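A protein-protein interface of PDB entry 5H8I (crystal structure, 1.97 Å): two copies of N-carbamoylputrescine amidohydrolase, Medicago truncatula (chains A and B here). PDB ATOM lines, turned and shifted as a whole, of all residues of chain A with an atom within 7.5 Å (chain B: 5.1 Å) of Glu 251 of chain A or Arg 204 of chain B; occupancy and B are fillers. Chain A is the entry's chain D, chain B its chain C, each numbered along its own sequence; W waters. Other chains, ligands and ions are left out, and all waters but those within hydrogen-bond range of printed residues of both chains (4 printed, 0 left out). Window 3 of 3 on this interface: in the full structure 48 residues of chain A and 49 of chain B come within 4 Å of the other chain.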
ATOM      1  N   ARG A 204      23.607  -5.117 -18.988  1.00  0.00           N
ATOM      2  CA  ARG A 204      23.384  -5.002 -20.435  1.00  0.00           C
ATOM      3  C   ARG A 204      24.659  -4.561 -21.180  1.00  0.00           C
ATOM      4  O   ARG A 204      24.980  -5.103 -22.248  1.00  0.00           O
ATOM      5  CB  ARG A 204      22.176  -4.105 -20.774  1.00  0.00           C
ATOM      6  CG  ARG A 204      20.861  -4.835 -20.602  1.00  0.00           C
ATOM      7  CD  ARG A 204      19.710  -4.065 -21.212  1.00  0.00           C
ATOM      8  NE  ARG A 204      19.531  -2.836 -20.488  1.00  0.00           N
ATOM      9  CZ  ARG A 204      18.614  -2.645 -19.526  1.00  0.00           C
ATOM     10  NH1 ARG A 204      17.769  -3.615 -19.200  1.00  0.00           N
ATOM     11  NH2 ARG A 204      18.537  -1.498 -18.924  1.00  0.00           N
ATOM     12  N   VAL A 205      25.385  -3.626 -20.595  1.00  0.00           N
ATOM     13  CA  VAL A 205      26.597  -3.110 -21.236  1.00  0.00           C
ATOM     14  C   VAL A 205      27.659  -4.206 -21.327  1.00  0.00           C
ATOM     15  O   VAL A 205      28.290  -4.377 -22.369  1.00  0.00           O
ATOM     16  CB  VAL A 205      27.076  -1.818 -20.526  1.00  0.00           C
ATOM     17  CG1 VAL A 205      28.435  -1.388 -21.013  1.00  0.00           C
ATOM     18  CG2 VAL A 205      26.071  -0.700 -20.789  1.00  0.00           C
ATOM     19  N   MET A 206      27.840  -4.975 -20.247  1.00  0.00           N
ATOM     20  CA  MET A 206      28.819  -6.069 -20.295  1.00  0.00           C
ATOM     21  C   MET A 206      28.372  -7.236 -21.222  1.00  0.00           C
ATOM     22  O   MET A 206      29.207  -7.833 -21.931  1.00  0.00           O
ATOM     23  CB  MET A 206      29.185  -6.591 -18.901  1.00  0.00           C
ATOM     24  CG  MET A 206      30.202  -5.718 -18.193  1.00  0.00           C
ATOM     25  SD  MET A 206      30.620  -6.358 -16.550  1.00  0.00           S
ATOM     26  CE  MET A 206      29.219  -5.715 -15.691  1.00  0.00           C
ATOM     27  N   GLN A 207      27.095  -7.548 -21.217  1.00  0.00           N
ATOM     28  CA  GLN A 207      26.576  -8.578 -22.123  1.00  0.00           C
ATOM     29  C   GLN A 207      26.874  -8.179 -23.562  1.00  0.00           C
ATOM     30  O   GLN A 207      27.191  -9.039 -24.396  1.00  0.00           O
ATOM     31  CB  GLN A 207      25.095  -8.780 -21.933  1.00  0.00           C
ATOM     32  CG  GLN A 207      24.727  -9.493 -20.631  1.00  0.00           C
ATOM     33  CD  GLN A 207      23.234  -9.512 -20.463  1.00  0.00           C
ATOM     34  OE1 GLN A 207      22.659  -8.554 -19.951  1.00  0.00           O
ATOM     35  NE2 GLN A 207      22.601 -10.578 -20.904  1.00  0.00           N
ATOM     36  N   GLY A 208      26.776  -6.873 -23.832  1.00  0.00           N
ATOM     37  CA  GLY A 208      27.170  -6.300 -25.131  1.00  0.00           C
ATOM     38  C   GLY A 208      28.611  -6.573 -25.527  1.00  0.00           C
ATOM     39  O   GLY A 208      28.856  -6.951 -26.667  1.00  0.00           O
ATOM     40  N   HIS A 209      29.539  -6.403 -24.597  1.00  0.00           N
ATOM     41  CA  HIS A 209      30.928  -6.685 -24.847  1.00  0.00           C
ATOM     42  C   HIS A 209      31.169  -8.156 -25.142  1.00  0.00           C
ATOM     43  O   HIS A 209      31.923  -8.483 -26.065  1.00  0.00           O
ATOM     44  CB  HIS A 209      31.846  -6.363 -23.678  1.00  0.00           C
ATOM     45  CG  HIS A 209      31.703  -4.994 -23.107  1.00  0.00           C
ATOM     46  ND1 HIS A 209      31.248  -3.897 -23.833  1.00  0.00           N
ATOM     47  CD2 HIS A 209      31.994  -4.536 -21.861  1.00  0.00           C
ATOM     48  CE1 HIS A 209      31.253  -2.827 -23.039  1.00  0.00           C
ATOM     49  NE2 HIS A 209      31.706  -3.190 -21.843  1.00  0.00           N
ATOM     50  N   ALA A 210      30.541  -9.042 -24.359  1.00  0.00           N
ATOM     51  CA  ALA A 210      30.706 -10.472 -24.564  1.00  0.00           C
ATOM     52  C   ALA A 210      30.193 -10.851 -25.964  1.00  0.00           C
ATOM     53  O   ALA A 210      30.845 -11.601 -26.687  1.00  0.00           O
ATOM     54  CB  ALA A 210      29.975 -11.269 -23.482  1.00  0.00           C
ATOM     55  N   GLY A 211      29.041 -10.308 -26.346  1.00  0.00           N
ATOM     56  CA  GLY A 211      28.461 -10.626 -27.621  1.00  0.00           C
ATOM     57  C   GLY A 211      29.191 -10.036 -28.806  1.00  0.00           C
ATOM     58  O   GLY A 211      29.228 -10.639 -29.867  1.00  0.00           O
ATOM     59  N   ALA A 212      29.768  -8.852 -28.627  1.00  0.00           N
ATOM     60  CA  ALA A 212      30.418  -8.147 -29.721  1.00  0.00           C
ATOM     61  C   ALA A 212      31.773  -8.714 -30.023  1.00  0.00           C
ATOM     62  O   ALA A 212      32.239  -8.644 -31.162  1.00  0.00           O
ATOM     63  CB  ALA A 212      30.510  -6.685 -29.451  1.00  0.00           C
ATOM     64  N   LEU A 217      32.549 -13.712 -20.312  1.00  0.00           N
ATOM     65  CA  LEU A 217      32.822 -12.591 -19.431  1.00  0.00           C
ATOM     66  C   LEU A 217      32.350 -12.902 -18.020  1.00  0.00           C
ATOM     67  O   LEU A 217      31.271 -13.461 -17.831  1.00  0.00           O
ATOM     68  CB  LEU A 217      32.166 -11.358 -19.992  1.00  0.00           C
ATOM     69  CG  LEU A 217      32.295 -10.019 -19.285  1.00  0.00           C
ATOM     70  CD1 LEU A 217      32.040  -8.904 -20.298  1.00  0.00           C
ATOM     71  CD2 LEU A 217      31.360  -9.879 -18.107  1.00  0.00           C
ATOM     72  N   PHE A 244      27.957 -12.253 -12.110  1.00  0.00           N
ATOM     73  CA  PHE A 244      27.475 -13.147 -13.144  1.00  0.00           C
ATOM     74  C   PHE A 244      28.569 -13.607 -14.088  1.00  0.00           C
ATOM     75  O   PHE A 244      29.680 -13.059 -14.101  1.00  0.00           O
ATOM     76  CB  PHE A 244      26.340 -12.455 -13.957  1.00  0.00           C
ATOM     77  CG  PHE A 244      26.804 -11.283 -14.805  1.00  0.00           C
ATOM     78  CD1 PHE A 244      27.271 -11.483 -16.083  1.00  0.00           C
ATOM     79  CD2 PHE A 244      26.777 -10.000 -14.315  1.00  0.00           C
ATOM     80  CE1 PHE A 244      27.704 -10.411 -16.876  1.00  0.00           C
ATOM     81  CE2 PHE A 244      27.203  -8.909 -15.086  1.00  0.00           C
ATOM     82  CZ  PHE A 244      27.673  -9.113 -16.375  1.00  0.00           C
ATOM     83  N   ILE A 245      28.220 -14.617 -14.887  1.00  0.00           N
ATOM     84  CA  ILE A 245      29.076 -15.140 -15.929  1.00  0.00           C
ATOM     85  C   ILE A 245      28.232 -15.156 -17.214  1.00  0.00           C
ATOM     86  O   ILE A 245      27.133 -15.734 -17.217  1.00  0.00           O
ATOM     87  CB  ILE A 245      29.590 -16.563 -15.597  1.00  0.00           C
ATOM     88  CG1 ILE A 245      30.332 -16.553 -14.241  1.00  0.00           C
ATOM     89  CG2 ILE A 245      30.459 -17.088 -16.744  1.00  0.00           C
ATOM     90  CD1 ILE A 245      30.634 -17.943 -13.705  1.00  0.00           C
ATOM     91  N   ALA A 246      28.746 -14.496 -18.272  1.00  0.00           N
ATOM     92  CA  ALA A 246      28.078 -14.445 -19.587  1.00  0.00           C
ATOM     93  C   ALA A 246      28.885 -15.263 -20.623  1.00  0.00           C
ATOM     94  O   ALA A 246      30.130 -15.329 -20.571  1.00  0.00           O
ATOM     95  CB  ALA A 246      27.920 -13.011 -20.038  1.00  0.00           C
ATOM     96  N   GLY A 247      28.156 -15.883 -21.534  1.00  0.00           N
ATOM     97  CA  GLY A 247      28.721 -16.668 -22.610  1.00  0.00           C
ATOM     98  C   GLY A 247      29.044 -15.763 -23.808  1.00  0.00           C
ATOM     99  O   GLY A 247      28.831 -14.547 -23.758  1.00  0.00           O
ATOM    100  N   PRO A 248      29.556 -16.357 -24.881  1.00  0.00           N
ATOM    101  CA  PRO A 248      30.072 -15.556 -25.985  1.00  0.00           C
ATOM    102  C   PRO A 248      29.003 -14.915 -26.868  1.00  0.00           C
ATOM    103  O   PRO A 248      29.378 -14.181 -27.801  1.00  0.00           O
ATOM    104  CB  PRO A 248      30.945 -16.572 -26.792  1.00  0.00           C
ATOM    105  CG  PRO A 248      30.321 -17.907 -26.486  1.00  0.00           C
ATOM    106  CD  PRO A 248      29.759 -17.807 -25.088  1.00  0.00           C
ATOM    107  N   THR A 249      27.722 -15.170 -26.612  1.00  0.00           N
ATOM    108  CA  THR A 249      26.664 -14.403 -27.277  1.00  0.00           C
ATOM    109  C   THR A 249      26.035 -13.373 -26.335  1.00  0.00           C
ATOM    110  O   THR A 249      25.020 -12.759 -26.696  1.00  0.00           O
ATOM    111  CB  THR A 249      25.526 -15.275 -27.868  1.00  0.00           C
ATOM    112  OG1 THR A 249      24.761 -15.901 -26.819  1.00  0.00           O
ATOM    113  CG2 THR A 249      26.088 -16.334 -28.859  1.00  0.00           C
ATOM    114  N   GLY A 250      26.627 -13.210 -25.146  1.00  0.00           N
ATOM    115  CA  GLY A 250      26.114 -12.309 -24.146  1.00  0.00           C
ATOM    116  C   GLY A 250      25.042 -12.906 -23.212  1.00  0.00           C
ATOM    117  O   GLY A 250      24.547 -12.211 -22.345  1.00  0.00           O
ATOM    118  N   GLU A 251      24.696 -14.175 -23.393  1.00  0.00           N
ATOM    119  CA  GLU A 251      23.701 -14.854 -22.552  1.00  0.00           C
ATOM    120  C   GLU A 251      24.266 -15.053 -21.129  1.00  0.00           C
ATOM    121  O   GLU A 251      25.409 -15.491 -20.967  1.00  0.00           O
ATOM    122  CB  GLU A 251      23.368 -16.218 -23.110  1.00  0.00           C
ATOM    123  CG  GLU A 251      22.256 -16.883 -22.348  1.00  0.00           C
ATOM    124  CD  GLU A 251      22.018 -18.353 -22.739  1.00  0.00           C
ATOM    125  OE1 GLU A 251      22.580 -18.812 -23.772  1.00  0.00           O
ATOM    126  OE2 GLU A 251      21.272 -19.042 -22.007  1.00  0.00           O
ATOM    127  N   ILE A 252      23.470 -14.738 -20.119  1.00  0.00           N
ATOM    128  CA  ILE A 252      23.870 -14.970 -18.752  1.00  0.00           C
ATOM    129  C   ILE A 252      23.806 -16.457 -18.495  1.00  0.00           C
ATOM    130  O   ILE A 252      22.759 -17.038 -18.630  1.00  0.00           O
ATOM    131  CB  ILE A 252      22.898 -14.312 -17.773  1.00  0.00           C
ATOM    132  CG1 ILE A 252      22.823 -12.793 -18.013  1.00  0.00           C
ATOM    133  CG2 ILE A 252      23.296 -14.602 -16.331  1.00  0.00           C
ATOM    134  CD1 ILE A 252      24.066 -12.036 -17.815  1.00  0.00           C
ATOM    135  N   VAL A 253      24.909 -17.083 -18.149  1.00  0.00           N
ATOM    136  CA  VAL A 253      24.852 -18.522 -17.848  1.00  0.00           C
ATOM    137  C   VAL A 253      24.758 -18.777 -16.357  1.00  0.00           C
ATOM    138  O   VAL A 253      24.270 -19.803 -15.948  1.00  0.00           O
ATOM    139  CB  VAL A 253      25.993 -19.330 -18.485  1.00  0.00           C
ATOM    140  CG1 VAL A 253      25.960 -19.165 -20.028  1.00  0.00           C
ATOM    141  CG2 VAL A 253      27.315 -18.918 -17.978  1.00  0.00           C
ATOM    142  N   SER A 254      25.208 -17.843 -15.547  1.00  0.00           N
ATOM    143  CA  SER A 254      25.060 -18.020 -14.127  1.00  0.00           C
ATOM    144  C   SER A 254      24.997 -16.643 -13.505  1.00  0.00           C
ATOM    145  O   SER A 254      25.728 -15.758 -13.912  1.00  0.00           O
ATOM    146  CB  SER A 254      26.248 -18.819 -13.614  1.00  0.00           C
ATOM    147  OG  SER A 254      26.255 -18.813 -12.198  1.00  0.00           O
ATOM    148  N   PHE A 268      33.715 -23.453 -20.070  1.00  0.00           N
ATOM    149  CA  PHE A 268      33.733 -22.968 -21.470  1.00  0.00           C
ATOM    150  C   PHE A 268      34.735 -23.785 -22.285  1.00  0.00           C
ATOM    151  O   PHE A 268      35.842 -24.073 -21.811  1.00  0.00           O
ATOM    152  CB  PHE A 268      34.074 -21.474 -21.556  1.00  0.00           C
ATOM    153  CG  PHE A 268      33.036 -20.613 -20.976  1.00  0.00           C
ATOM    154  CD1 PHE A 268      31.820 -20.467 -21.621  1.00  0.00           C
ATOM    155  CD2 PHE A 268      33.245 -19.938 -19.736  1.00  0.00           C
ATOM    156  CE1 PHE A 268      30.815 -19.654 -21.092  1.00  0.00           C
ATOM    157  CE2 PHE A 268      32.230 -19.139 -19.197  1.00  0.00           C
ATOM    158  CZ  PHE A 268      31.013 -18.992 -19.892  1.00  0.00           C
ATOM    159  N   ASP B 200      18.697 -13.381 -30.369  1.00  0.00           N
ATOM    160  CA  ASP B 200      18.978 -12.920 -29.012  1.00  0.00           C
ATOM    161  C   ASP B 200      20.374 -12.258 -28.930  1.00  0.00           C
ATOM    162  O   ASP B 200      20.519 -11.255 -28.280  1.00  0.00           O
ATOM    163  CB  ASP B 200      18.909 -14.052 -28.003  1.00  0.00           C
ATOM    164  CG  ASP B 200      17.495 -14.573 -27.803  1.00  0.00           C
ATOM    165  OD1 ASP B 200      16.520 -13.820 -28.053  1.00  0.00           O
ATOM    166  OD2 ASP B 200      17.364 -15.729 -27.393  1.00  0.00           O
ATOM    167  N   HIS B 201      21.363 -12.853 -29.615  1.00  0.00           N
ATOM    168  CA  HIS B 201      22.700 -12.321 -29.720  1.00  0.00           C
ATOM    169  C   HIS B 201      22.670 -10.934 -30.364  1.00  0.00           C
ATOM    170  O   HIS B 201      23.283  -9.961 -29.839  1.00  0.00           O
ATOM    171  CB  HIS B 201      23.537 -13.300 -30.548  1.00  0.00           C
ATOM    172  CG  HIS B 201      24.983 -12.980 -30.633  1.00  0.00           C
ATOM    173  ND1 HIS B 201      25.806 -13.611 -31.533  1.00  0.00           N
ATOM    174  CD2 HIS B 201      25.767 -12.111 -29.950  1.00  0.00           C
ATOM    175  CE1 HIS B 201      27.037 -13.144 -31.399  1.00  0.00           C
ATOM    176  NE2 HIS B 201      27.039 -12.237 -30.448  1.00  0.00           N
ATOM    177  N   TRP B 202      21.935 -10.855 -31.466  1.00  0.00           N
ATOM    178  CA  TRP B 202      21.748  -9.641 -32.239  1.00  0.00           C
ATOM    179  C   TRP B 202      21.217  -8.481 -31.376  1.00  0.00           C
ATOM    180  O   TRP B 202      21.794  -7.367 -31.394  1.00  0.00           O
ATOM    181  CB  TRP B 202      20.821  -9.951 -33.410  1.00  0.00           C
ATOM    182  CG  TRP B 202      20.346  -8.862 -34.290  1.00  0.00           C
ATOM    183  CD1 TRP B 202      21.051  -8.194 -35.261  1.00  0.00           C
ATOM    184  CD2 TRP B 202      19.020  -8.341 -34.338  1.00  0.00           C
ATOM    185  NE1 TRP B 202      20.234  -7.258 -35.896  1.00  0.00           N
ATOM    186  CE2 TRP B 202      18.984  -7.340 -35.342  1.00  0.00           C
ATOM    187  CE3 TRP B 202      17.844  -8.616 -33.620  1.00  0.00           C
ATOM    188  CZ2 TRP B 202      17.834  -6.630 -35.631  1.00  0.00           C
ATOM    189  CZ3 TRP B 202      16.697  -7.888 -33.918  1.00  0.00           C
ATOM    190  CH2 TRP B 202      16.707  -6.912 -34.906  1.00  0.00           C
ATOM    191  N   LYS B 203      20.151  -8.747 -30.630  1.00  0.00           N
ATOM    192  CA  LYS B 203      19.584  -7.737 -29.733  1.00  0.00           C
ATOM    193  C   LYS B 203      20.541  -7.314 -28.642  1.00  0.00           C
ATOM    194  O   LYS B 203      20.690  -6.125 -28.393  1.00  0.00           O
ATOM    195  CB  LYS B 203      18.273  -8.239 -29.087  1.00  0.00           C
ATOM    196  CG  LYS B 203      17.099  -8.127 -30.029  1.00  0.00           C
ATOM    197  CD  LYS B 203      15.792  -8.632 -29.422  1.00  0.00           C
ATOM    198  CE  LYS B 203      15.646 -10.147 -29.500  1.00  0.00           C
ATOM    199  NZ  LYS B 203      14.252 -10.548 -29.102  1.00  0.00           N
ATOM    200  N   ARG B 204      21.171  -8.284 -27.978  1.00  0.00           N
ATOM    201  CA  ARG B 204      22.088  -7.973 -26.859  1.00  0.00           C
ATOM    202  C   ARG B 204      23.259  -7.061 -27.278  1.00  0.00           C
ATOM    203  O   ARG B 204      23.662  -6.186 -26.550  1.00  0.00           O
ATOM    204  CB  ARG B 204      22.596  -9.268 -26.194  1.00  0.00           C
ATOM    205  CG  ARG B 204      21.549  -9.976 -25.354  1.00  0.00           C
ATOM    206  CD  ARG B 204      22.159 -11.064 -24.488  1.00  0.00           C
ATOM    207  NE  ARG B 204      22.566 -12.181 -25.320  1.00  0.00           N
ATOM    208  CZ  ARG B 204      21.864 -13.309 -25.470  1.00  0.00           C
ATOM    209  NH1 ARG B 204      20.718 -13.482 -24.814  1.00  0.00           N
ATOM    210  NH2 ARG B 204      22.315 -14.263 -26.254  1.00  0.00           N
ATOM    211  N   VAL B 205      23.791  -7.257 -28.468  1.00  0.00           N
ATOM    212  CA  VAL B 205      24.915  -6.454 -28.896  1.00  0.00           C
ATOM    213  C   VAL B 205      24.490  -5.004 -29.083  1.00  0.00           C
ATOM    214  O   VAL B 205      25.214  -4.063 -28.662  1.00  0.00           O
ATOM    215  CB  VAL B 205      25.581  -7.046 -30.163  1.00  0.00           C
ATOM    216  CG1 VAL B 205      26.553  -6.069 -30.799  1.00  0.00           C
ATOM    217  CG2 VAL B 205      26.312  -8.322 -29.765  1.00  0.00           C
ATOM    218  N   MET B 206      23.323  -4.808 -29.703  1.00  0.00           N
ATOM    219  CA  MET B 206      22.829  -3.452 -29.904  1.00  0.00           C
ATOM    220  C   MET B 206      22.360  -2.811 -28.597  1.00  0.00           C
ATOM    221  O   MET B 206      22.533  -1.624 -28.406  1.00  0.00           O
ATOM    222  CB  MET B 206      21.709  -3.425 -30.929  1.00  0.00           C
ATOM    223  CG  MET B 206      22.210  -3.391 -32.384  1.00  0.00           C
ATOM    224  SD  MET B 206      20.789  -3.229 -33.495  1.00  0.00           S
ATOM    225  CE  MET B 206      20.222  -4.916 -33.476  1.00  0.00           C
ATOM    226  N   GLN B 207      21.770  -3.594 -27.709  1.00  0.00           N
ATOM    227  CA  GLN B 207      21.414  -3.076 -26.376  1.00  0.00           C
ATOM    228  C   GLN B 207      22.649  -2.581 -25.661  1.00  0.00           C
ATOM    229  O   GLN B 207      22.589  -1.630 -24.954  1.00  0.00           O
ATOM    230  CB  GLN B 207      20.712  -4.118 -25.529  1.00  0.00           C
ATOM    231  CG  GLN B 207      19.286  -4.391 -25.965  1.00  0.00           C
ATOM    232  CD  GLN B 207      18.687  -5.511 -25.176  1.00  0.00           C
ATOM    233  OE1 GLN B 207      18.836  -6.660 -25.533  1.00  0.00           O
ATOM    234  NE2 GLN B 207      18.003  -5.185 -24.108  1.00  0.00           N
ATOM    235  N   GLY B 208      23.768  -3.248 -25.854  1.00  0.00           N
ATOM    236  CA  GLY B 208      25.017  -2.819 -25.254  1.00  0.00           C
ATOM    237  C   GLY B 208      25.482  -1.475 -25.804  1.00  0.00           C
ATOM    238  O   GLY B 208      25.993  -0.668 -25.050  1.00  0.00           O
HETATM  239  O   HOH W   1      23.102  -6.346 -23.876  1.00  0.00           O
HETATM  240  O   HOH W   2      28.352  -2.512 -24.730  1.00  0.00           O
HETATM  241  O   HOH W   3      22.043 -16.558 -27.716  1.00  0.00           O
HETATM  242  O   HOH W   4      27.967  -4.330 -27.726  1.00  0.00           O
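Water W3 bridges the guanidinium group of Arg 204 of chain B and the side-chain hydroxyl of Thr 249 of chain A. Water W1 bridges the backbone carbonyl oxygen (O) of Arg 204 of chain B (2.7 Å) and the backbone carbonyl oxygen (O) of Arg 204 of chain A (2.8 Å). Water W4 lies within hydrogen-bond range of the backbone carbonyl oxygen of Val 205 of chain B (2.9 Å) and the backbone carbonyl oxygen of Gly 208 of chain A (3.0 Å). Water W2 lies within hydrogen-bond range of the backbone carbonyl oxygen (O) of Val 205 of chain A (3.0 Å), the backbone carbonyl oxygen (O) of Gly 208 of chain B (3.0 Å) and a ring nitrogen (ND1) of His 209 of chain A (3.3 Å).
The side-chain amide oxygen (OE1) of Gln 207 of chain B sits close to the backbone carbonyl oxygen (O) of Lys 203 of chain B, at 3.5 Å. The backbone carbonyl oxygen (O) of Gly 250 of chain A sits at hydrogen-bond distance from the side-chain amide nitrogen (NE2) of Gln 207 of chain A, 2.9 Å away.
O of Gly 211 of chain A is in hydrogen-bond range of NE2 of His 201 of chain B (2.8 Å). NE of Arg 204 of chain B is in hydrogen-bond range of O of Thr 249 of chain A, at 2.9 Å. The backbone NH (N) of Glu 251 of chain A lies close to the guanidinium group (NE) of Arg 204 of chain B (3.5 Å).
Among the printed residues, merely in contact across the chains: Gly 250 of chain A with Arg 204 of chain B, Thr 249 of chain A with His 201 of chain B, Gly 211 of chain A with Val 205 of chain B, Arg 204 of chain A with Gln 207 of chain B, Gln 207 of chain A with Arg 204 of chain B, Ala 212 of chain A with Val 205 of chain B, Arg 204 of chain A with Gly 208 of chain B and Gly 208 of chain A with Arg 204 of chain B.
Arg 204 of chain A touches Gln 207 of chain B, and with the chains exchanged Gln 207 of chain A touches Arg 204 of chain B. Arg 204 of chain A touches Gly 208 of chain B, and with the chains exchanged Gly 208 of chain A touches Arg 204 of chain B. Of the 11 pairs that touch across the chains among the printed residues, 4 have their exchanged pair printed and touching as well.
Of the printed residues of chain B, Gly 208 of chain A touches Arg 204. Printed residues of chain B within 4 Å of Gly 250 of chain A: Arg 204. Of chain B, only Arg 204 (3.5 Å) comes within 4 Å of Glu 251 of chain A. Of the printed residues of chain A, His 201 of chain B touches Gly 211 (2.8 Å) and Thr 249 (3.4 Å). Of the printed residues of chain A, Val 205 of chain B touches Gly 211 (3.5 Å) and Ala 212 (3.7 Å). The nearest printed residue of chain B that does not touch Glu 251 of chain A is His 201 of chain B (6.9 Å). The nearest residue of chain A that does not touch Arg 204 of chain B is Arg 204 of chain A (4.6 Å).
Of the 9 printed residues of chain B, 5 touch a printed residue of chain A. Printed residues of chain B that touch a printed residue of chain A: His 201, Arg 204, Val 205, Gln 207 and Gly 208. Printed residues of chain A that touch a printed residue of chain B: Arg 204, Gln 207, Gly 208, Gly 211, Ala 212, Thr 249, Gly 250 and Glu 251. Among the printed residues, 11 pairs touch across the chains.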
